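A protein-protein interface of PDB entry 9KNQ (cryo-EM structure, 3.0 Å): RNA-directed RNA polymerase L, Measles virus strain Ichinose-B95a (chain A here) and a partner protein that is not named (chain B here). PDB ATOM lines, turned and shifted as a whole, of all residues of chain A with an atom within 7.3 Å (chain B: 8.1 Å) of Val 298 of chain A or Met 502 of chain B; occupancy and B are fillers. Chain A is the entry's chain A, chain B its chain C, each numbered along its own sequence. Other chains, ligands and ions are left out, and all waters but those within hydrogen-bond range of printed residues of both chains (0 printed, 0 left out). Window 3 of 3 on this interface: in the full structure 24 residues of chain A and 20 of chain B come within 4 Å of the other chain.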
ATOM      1  N   ASP A 295      22.810  30.848  -2.881  1.00  0.00           N
ATOM      2  CA  ASP A 295      21.493  31.400  -3.150  1.00  0.00           C
ATOM      3  C   ASP A 295      20.526  30.303  -3.590  1.00  0.00           C
ATOM      4  O   ASP A 295      20.904  29.151  -3.819  1.00  0.00           O
ATOM      5  CB  ASP A 295      21.581  32.489  -4.214  1.00  0.00           C
ATOM      6  CG  ASP A 295      20.469  33.503  -4.096  1.00  0.00           C
ATOM      7  OD1 ASP A 295      19.338  33.101  -3.760  1.00  0.00           O
ATOM      8  OD2 ASP A 295      20.723  34.699  -4.338  1.00  0.00           O
ATOM      9  N   ILE A 296      19.254  30.679  -3.710  1.00  0.00           N
ATOM     10  CA  ILE A 296      18.205  29.743  -4.087  1.00  0.00           C
ATOM     11  C   ILE A 296      17.726  29.941  -5.520  1.00  0.00           C
ATOM     12  O   ILE A 296      17.180  28.995  -6.107  1.00  0.00           O
ATOM     13  CB  ILE A 296      17.013  29.818  -3.110  1.00  0.00           C
ATOM     14  CG1 ILE A 296      16.162  28.553  -3.197  1.00  0.00           C
ATOM     15  CG2 ILE A 296      16.165  31.037  -3.396  1.00  0.00           C
ATOM     16  CD1 ILE A 296      16.934  27.286  -2.951  1.00  0.00           C
ATOM     17  N   THR A 297      17.913  31.121  -6.103  1.00  0.00           N
ATOM     18  CA  THR A 297      17.601  31.363  -7.509  1.00  0.00           C
ATOM     19  C   THR A 297      18.913  31.242  -8.272  1.00  0.00           C
ATOM     20  O   THR A 297      19.740  32.157  -8.254  1.00  0.00           O
ATOM     21  CB  THR A 297      16.955  32.727  -7.709  1.00  0.00           C
ATOM     22  OG1 THR A 297      17.847  33.572  -8.444  1.00  0.00           O
ATOM     23  CG2 THR A 297      16.648  33.368  -6.371  1.00  0.00           C
ATOM     24  N   VAL A 298      19.090  30.111  -8.957  1.00  0.00           N
ATOM     25  CA  VAL A 298      20.401  29.698  -9.442  1.00  0.00           C
ATOM     26  C   VAL A 298      21.033  30.719 -10.378  1.00  0.00           C
ATOM     27  O   VAL A 298      22.263  30.777 -10.484  1.00  0.00           O
ATOM     28  CB  VAL A 298      20.280  28.316 -10.117  1.00  0.00           C
ATOM     29  CG1 VAL A 298      19.381  28.395 -11.335  1.00  0.00           C
ATOM     30  CG2 VAL A 298      21.647  27.765 -10.471  1.00  0.00           C
ATOM     31  N   GLU A 299      20.233  31.548 -11.047  1.00  0.00           N
ATOM     32  CA  GLU A 299      20.801  32.523 -11.970  1.00  0.00           C
ATOM     33  C   GLU A 299      21.607  33.608 -11.272  1.00  0.00           C
ATOM     34  O   GLU A 299      22.308  34.365 -11.950  1.00  0.00           O
ATOM     35  CB  GLU A 299      19.695  33.169 -12.805  1.00  0.00           C
ATOM     36  CG  GLU A 299      18.870  32.185 -13.611  1.00  0.00           C
ATOM     37  CD  GLU A 299      17.562  31.830 -12.935  1.00  0.00           C
ATOM     38  OE1 GLU A 299      16.512  32.360 -13.354  1.00  0.00           O
ATOM     39  OE2 GLU A 299      17.583  31.024 -11.982  1.00  0.00           O
ATOM     40  N   LEU A 300      21.529  33.705  -9.947  1.00  0.00           N
ATOM     41  CA  LEU A 300      22.232  34.751  -9.219  1.00  0.00           C
ATOM     42  C   LEU A 300      23.633  34.351  -8.784  1.00  0.00           C
ATOM     43  O   LEU A 300      24.448  35.231  -8.491  1.00  0.00           O
ATOM     44  CB  LEU A 300      21.427  35.167  -7.985  1.00  0.00           C
ATOM     45  CG  LEU A 300      20.238  36.085  -8.249  1.00  0.00           C
ATOM     46  CD1 LEU A 300      19.485  36.362  -6.965  1.00  0.00           C
ATOM     47  CD2 LEU A 300      20.709  37.377  -8.881  1.00  0.00           C
ATOM     48  N   ARG A 301      23.932  33.055  -8.729  1.00  0.00           N
ATOM     49  CA  ARG A 301      25.215  32.586  -8.222  1.00  0.00           C
ATOM     50  C   ARG A 301      26.376  33.051  -9.091  1.00  0.00           C
ATOM     51  O   ARG A 301      26.489  32.652 -10.252  1.00  0.00           O
ATOM     52  CB  ARG A 301      25.213  31.061  -8.124  1.00  0.00           C
ATOM     53  CG  ARG A 301      24.063  30.506  -7.313  1.00  0.00           C
ATOM     54  CD  ARG A 301      24.289  29.052  -6.959  1.00  0.00           C
ATOM     55  NE  ARG A 301      23.196  28.513  -6.160  1.00  0.00           N
ATOM     56  CZ  ARG A 301      23.251  27.360  -5.505  1.00  0.00           C
ATOM     57  NH1 ARG A 301      24.351  26.625  -5.551  1.00  0.00           N
ATOM     58  NH2 ARG A 301      22.209  26.943  -4.802  1.00  0.00           N
ATOM     59  N   GLY A 302      27.247  33.893  -8.536  1.00  0.00           N
ATOM     60  CA  GLY A 302      28.455  34.314  -9.215  1.00  0.00           C
ATOM     61  C   GLY A 302      28.448  35.734  -9.733  1.00  0.00           C
ATOM     62  O   GLY A 302      29.467  36.176 -10.278  1.00  0.00           O
ATOM     63  N   ARG A 794      11.810  32.767  -6.311  1.00  0.00           N
ATOM     64  CA  ARG A 794      12.196  33.013  -7.695  1.00  0.00           C
ATOM     65  C   ARG A 794      11.403  34.169  -8.292  1.00  0.00           C
ATOM     66  O   ARG A 794      11.971  35.036  -8.971  1.00  0.00           O
ATOM     67  CB  ARG A 794      12.004  31.741  -8.516  1.00  0.00           C
ATOM     68  CG  ARG A 794      12.853  31.671  -9.770  1.00  0.00           C
ATOM     69  CD  ARG A 794      13.008  30.236 -10.248  1.00  0.00           C
ATOM     70  NE  ARG A 794      13.968  29.486  -9.443  1.00  0.00           N
ATOM     71  CZ  ARG A 794      13.635  28.598  -8.511  1.00  0.00           C
ATOM     72  NH1 ARG A 794      12.360  28.346  -8.258  1.00  0.00           N
ATOM     73  NH2 ARG A 794      14.577  27.962  -7.830  1.00  0.00           N
ATOM     74  N   GLY B 451      22.493  39.140 -13.489  1.00  0.00           N
ATOM     75  CA  GLY B 451      22.723  37.717 -13.648  1.00  0.00           C
ATOM     76  C   GLY B 451      24.109  37.493 -14.204  1.00  0.00           C
ATOM     77  O   GLY B 451      24.779  38.418 -14.666  1.00  0.00           O
ATOM     78  N   PHE B 452      24.537  36.238 -14.157  1.00  0.00           N
ATOM     79  CA  PHE B 452      25.871  35.854 -14.593  1.00  0.00           C
ATOM     80  C   PHE B 452      25.782  35.067 -15.891  1.00  0.00           C
ATOM     81  O   PHE B 452      25.015  34.104 -15.985  1.00  0.00           O
ATOM     82  CB  PHE B 452      26.578  35.027 -13.521  1.00  0.00           C
ATOM     83  CG  PHE B 452      27.733  34.232 -14.041  1.00  0.00           C
ATOM     84  CD1 PHE B 452      28.883  34.863 -14.471  1.00  0.00           C
ATOM     85  CD2 PHE B 452      27.666  32.853 -14.108  1.00  0.00           C
ATOM     86  CE1 PHE B 452      29.947  34.138 -14.953  1.00  0.00           C
ATOM     87  CE2 PHE B 452      28.727  32.122 -14.591  1.00  0.00           C
ATOM     88  CZ  PHE B 452      29.867  32.766 -15.016  1.00  0.00           C
ATOM     89  N   PRO B 454      28.704  33.444 -18.780  1.00  0.00           N
ATOM     90  CA  PRO B 454      30.140  33.289 -19.029  1.00  0.00           C
ATOM     91  C   PRO B 454      30.567  34.007 -20.300  1.00  0.00           C
ATOM     92  O   PRO B 454      29.752  34.471 -21.099  1.00  0.00           O
ATOM     93  CB  PRO B 454      30.319  31.773 -19.158  1.00  0.00           C
ATOM     94  CG  PRO B 454      29.088  31.182 -18.545  1.00  0.00           C
ATOM     95  CD  PRO B 454      27.998  32.156 -18.824  1.00  0.00           C
ATOM     96  N   ILE B 467      31.758  27.729  -8.525  1.00  0.00           N
ATOM     97  CA  ILE B 467      30.396  27.213  -8.410  1.00  0.00           C
ATOM     98  C   ILE B 467      30.418  25.702  -8.230  1.00  0.00           C
ATOM     99  O   ILE B 467      29.727  25.147  -7.364  1.00  0.00           O
ATOM    100  CB  ILE B 467      29.558  27.623  -9.632  1.00  0.00           C
ATOM    101  CG1 ILE B 467      29.323  29.130  -9.639  1.00  0.00           C
ATOM    102  CG2 ILE B 467      28.235  26.892  -9.631  1.00  0.00           C
ATOM    103  CD1 ILE B 467      28.431  29.597 -10.760  1.00  0.00           C
ATOM    104  N   ALA B 495      28.702  28.544 -22.592  1.00  0.00           N
ATOM    105  CA  ALA B 495      27.354  28.895 -22.161  1.00  0.00           C
ATOM    106  C   ALA B 495      26.475  27.658 -22.041  1.00  0.00           C
ATOM    107  O   ALA B 495      25.668  27.547 -21.110  1.00  0.00           O
ATOM    108  CB  ALA B 495      26.739  29.901 -23.131  1.00  0.00           C
ATOM    109  N   LYS B 496      26.618  26.713 -22.973  1.00  0.00           N
ATOM    110  CA  LYS B 496      25.832  25.487 -22.904  1.00  0.00           C
ATOM    111  C   LYS B 496      26.195  24.669 -21.673  1.00  0.00           C
ATOM    112  O   LYS B 496      25.314  24.133 -20.988  1.00  0.00           O
ATOM    113  CB  LYS B 496      26.036  24.663 -24.173  1.00  0.00           C
ATOM    114  CG  LYS B 496      25.329  23.320 -24.159  1.00  0.00           C
ATOM    115  CD  LYS B 496      25.731  22.475 -25.355  1.00  0.00           C
ATOM    116  CE  LYS B 496      25.537  23.234 -26.656  1.00  0.00           C
ATOM    117  NZ  LYS B 496      24.130  23.685 -26.834  1.00  0.00           N
ATOM    118  N   PHE B 497      27.491  24.562 -21.376  1.00  0.00           N
ATOM    119  CA  PHE B 497      27.917  23.841 -20.186  1.00  0.00           C
ATOM    120  C   PHE B 497      27.392  24.510 -18.924  1.00  0.00           C
ATOM    121  O   PHE B 497      26.979  23.830 -17.982  1.00  0.00           O
ATOM    122  CB  PHE B 497      29.441  23.741 -20.145  1.00  0.00           C
ATOM    123  CG  PHE B 497      29.960  22.926 -19.000  1.00  0.00           C
ATOM    124  CD1 PHE B 497      29.953  21.546 -19.058  1.00  0.00           C
ATOM    125  CD2 PHE B 497      30.453  23.539 -17.865  1.00  0.00           C
ATOM    126  CE1 PHE B 497      30.429  20.794 -18.007  1.00  0.00           C
ATOM    127  CE2 PHE B 497      30.929  22.792 -16.812  1.00  0.00           C
ATOM    128  CZ  PHE B 497      30.917  21.419 -16.882  1.00  0.00           C
ATOM    129  N   HIS B 498      27.401  25.844 -18.888  1.00  0.00           N
ATOM    130  CA  HIS B 498      26.853  26.550 -17.734  1.00  0.00           C
ATOM    131  C   HIS B 498      25.362  26.285 -17.581  1.00  0.00           C
ATOM    132  O   HIS B 498      24.873  26.049 -16.469  1.00  0.00           O
ATOM    133  CB  HIS B 498      27.118  28.049 -17.860  1.00  0.00           C
ATOM    134  CG  HIS B 498      26.463  28.870 -16.794  1.00  0.00           C
ATOM    135  ND1 HIS B 498      25.304  29.582 -17.011  1.00  0.00           N
ATOM    136  CD2 HIS B 498      26.803  29.088 -15.502  1.00  0.00           C
ATOM    137  CE1 HIS B 498      24.960  30.207 -15.900  1.00  0.00           C
ATOM    138  NE2 HIS B 498      25.853  29.924 -14.969  1.00  0.00           N
ATOM    139  N   GLN B 499      24.621  26.326 -18.690  1.00  0.00           N
ATOM    140  CA  GLN B 499      23.182  26.098 -18.628  1.00  0.00           C
ATOM    141  C   GLN B 499      22.858  24.675 -18.199  1.00  0.00           C
ATOM    142  O   GLN B 499      21.852  24.448 -17.521  1.00  0.00           O
ATOM    143  CB  GLN B 499      22.543  26.407 -19.979  1.00  0.00           C
ATOM    144  CG  GLN B 499      22.468  27.889 -20.292  1.00  0.00           C
ATOM    145  CD  GLN B 499      22.098  28.165 -21.734  1.00  0.00           C
ATOM    146  OE1 GLN B 499      21.953  27.243 -22.537  1.00  0.00           O
ATOM    147  NE2 GLN B 499      21.946  29.439 -22.072  1.00  0.00           N
ATOM    148  N   MET B 500      23.693  23.707 -18.581  1.00  0.00           N
ATOM    149  CA  MET B 500      23.488  22.344 -18.105  1.00  0.00           C
ATOM    150  C   MET B 500      23.848  22.216 -16.630  1.00  0.00           C
ATOM    151  O   MET B 500      23.131  21.561 -15.860  1.00  0.00           O
ATOM    152  CB  MET B 500      24.311  21.370 -18.944  1.00  0.00           C
ATOM    153  CG  MET B 500      24.196  19.929 -18.492  1.00  0.00           C
ATOM    154  SD  MET B 500      25.580  18.919 -19.042  1.00  0.00           S
ATOM    155  CE  MET B 500      26.931  19.707 -18.172  1.00  0.00           C
ATOM    156  N   LEU B 501      24.958  22.837 -16.224  1.00  0.00           N
ATOM    157  CA  LEU B 501      25.406  22.770 -14.839  1.00  0.00           C
ATOM    158  C   LEU B 501      24.373  23.362 -13.895  1.00  0.00           C
ATOM    159  O   LEU B 501      24.198  22.874 -12.773  1.00  0.00           O
ATOM    160  CB  LEU B 501      26.738  23.501 -14.699  1.00  0.00           C
ATOM    161  CG  LEU B 501      27.316  23.629 -13.295  1.00  0.00           C
ATOM    162  CD1 LEU B 501      27.743  22.268 -12.792  1.00  0.00           C
ATOM    163  CD2 LEU B 501      28.483  24.596 -13.294  1.00  0.00           C
ATOM    164  N   MET B 502      23.692  24.425 -14.326  1.00  0.00           N
ATOM    165  CA  MET B 502      22.646  25.014 -13.497  1.00  0.00           C
ATOM    166  C   MET B 502      21.595  23.976 -13.132  1.00  0.00           C
ATOM    167  O   MET B 502      21.270  23.789 -11.952  1.00  0.00           O
ATOM    168  CB  MET B 502      22.003  26.196 -14.221  1.00  0.00           C
ATOM    169  CG  MET B 502      22.633  27.537 -13.903  1.00  0.00           C
ATOM    170  SD  MET B 502      21.980  28.861 -14.935  1.00  0.00           S
ATOM    171  CE  MET B 502      20.238  28.451 -14.944  1.00  0.00           C
ATOM    172  N   LYS B 503      21.051  23.291 -14.139  1.00  0.00           N
ATOM    173  CA  LYS B 503      20.071  22.242 -13.886  1.00  0.00           C
ATOM    174  C   LYS B 503      20.658  21.151 -13.004  1.00  0.00           C
ATOM    175  O   LYS B 503      20.025  20.712 -12.036  1.00  0.00           O
ATOM    176  CB  LYS B 503      19.585  21.650 -15.208  1.00  0.00           C
ATOM    177  CG  LYS B 503      18.945  22.653 -16.145  1.00  0.00           C
ATOM    178  CD  LYS B 503      18.422  21.964 -17.394  1.00  0.00           C
ATOM    179  CE  LYS B 503      17.776  22.955 -18.345  1.00  0.00           C
ATOM    180  NZ  LYS B 503      17.284  22.289 -19.583  1.00  0.00           N
ATOM    181  N   ILE B 504      21.880  20.711 -13.316  1.00  0.00           N
ATOM    182  CA  ILE B 504      22.477  19.600 -12.580  1.00  0.00           C
ATOM    183  C   ILE B 504      22.594  19.929 -11.097  1.00  0.00           C
ATOM    184  O   ILE B 504      22.337  19.077 -10.238  1.00  0.00           O
ATOM    185  CB  ILE B 504      23.843  19.226 -13.186  1.00  0.00           C
ATOM    186  CG1 ILE B 504      23.677  18.747 -14.628  1.00  0.00           C
ATOM    187  CG2 ILE B 504      24.515  18.150 -12.357  1.00  0.00           C
ATOM    188  CD1 ILE B 504      24.984  18.418 -15.309  1.00  0.00           C
ATOM    189  N   ILE B 505      22.969  21.167 -10.769  1.00  0.00           N
ATOM    190  CA  ILE B 505      23.237  21.487  -9.371  1.00  0.00           C
ATOM    191  C   ILE B 505      21.963  21.870  -8.630  1.00  0.00           C
ATOM    192  O   ILE B 505      21.823  21.573  -7.440  1.00  0.00           O
ATOM    193  CB  ILE B 505      24.310  22.585  -9.248  1.00  0.00           C
ATOM    194  CG1 ILE B 505      23.782  23.931  -9.744  1.00  0.00           C
ATOM    195  CG2 ILE B 505      25.573  22.181  -9.976  1.00  0.00           C
ATOM    196  CD1 ILE B 505      24.758  25.063  -9.563  1.00  0.00           C
ATOM    197  N   MET B 506      21.013  22.531  -9.293  1.00  0.00           N
ATOM    198  CA  MET B 506      19.840  22.981  -8.555  1.00  0.00           C
ATOM    199  C   MET B 506      18.712  21.957  -8.572  1.00  0.00           C
ATOM    200  O   MET B 506      17.734  22.126  -7.836  1.00  0.00           O
ATOM    201  CB  MET B 506      19.358  24.337  -9.078  1.00  0.00           C
ATOM    202  CG  MET B 506      18.557  24.333 -10.375  1.00  0.00           C
ATOM    203  SD  MET B 506      16.789  24.042 -10.146  1.00  0.00           S
ATOM    204  CE  MET B 506      16.230  23.977 -11.843  1.00  0.00           C
ATOM    205  N   LYS B 507      18.823  20.902  -9.375  1.00  0.00           N
ATOM    206  CA  LYS B 507      17.845  19.823  -9.344  1.00  0.00           C
ATOM    207  C   LYS B 507      17.853  19.124  -7.988  1.00  0.00           C
ATOM    208  O   LYS B 507      16.900  18.441  -7.617  1.00  0.00           O
ATOM    209  CB  LYS B 507      18.119  18.808 -10.455  1.00  0.00           C
ATOM    210  CG  LYS B 507      17.297  19.020 -11.715  1.00  0.00           C
ATOM    211  CD  LYS B 507      17.345  17.792 -12.612  1.00  0.00           C
ATOM    212  CE  LYS B 507      16.336  17.892 -13.744  1.00  0.00           C
ATOM    213  NZ  LYS B 507      16.310  16.656 -14.573  1.00  0.00           N
ATOM    214  OXT LYS B 507      18.815  19.228  -7.228  1.00  0.00           O
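The backbone carbonyl oxygen (O) of Asp 295 of chain A sits at hydrogen-bond distance from the guanidinium group (NH2) of Arg 301 of chain A (2.7 Å).
Val 298 of chain A touches Met 502 of chain B (CG2 to CG, 3.6 Å). Glu 299 of chain A touches Gly 451 of chain B (O to CA, 3.8 Å). Phe 452 of chain B touches Glu 299 of chain A. O of Arg 301 of chain A touches CD1 of Ile 467 of chain B, at 3.7 Å.
Val 298 of chain A touches just one residue of chain B: Met 502 (3.6 Å). Of chain A, only Val 298 comes within 4 Å of Met 502 of chain B. Printed residues of chain A within 4 Å of Ile 467 of chain B: Arg 301 (3.7 Å). Printed residues of chain B within 4 Å of Glu 299 of chain A: Gly 451 and Phe 452. Gly 302 of chain A touches none of the printed residues of chain B.
Printed residues of chain A that touch a printed residue of chain B: Val 298, Glu 299 and Arg 301. Of the 17 printed residues of chain B, 4 touch a printed residue of chain A. Hydrophobic or aromatic side chains of chain B that line the printed part of chain A: Ile 467 and Met 502. Among the printed residues, no Asp or Glu carboxylate lies within 4 Å of a Lys or Arg side-chain nitrogen of the other chain.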
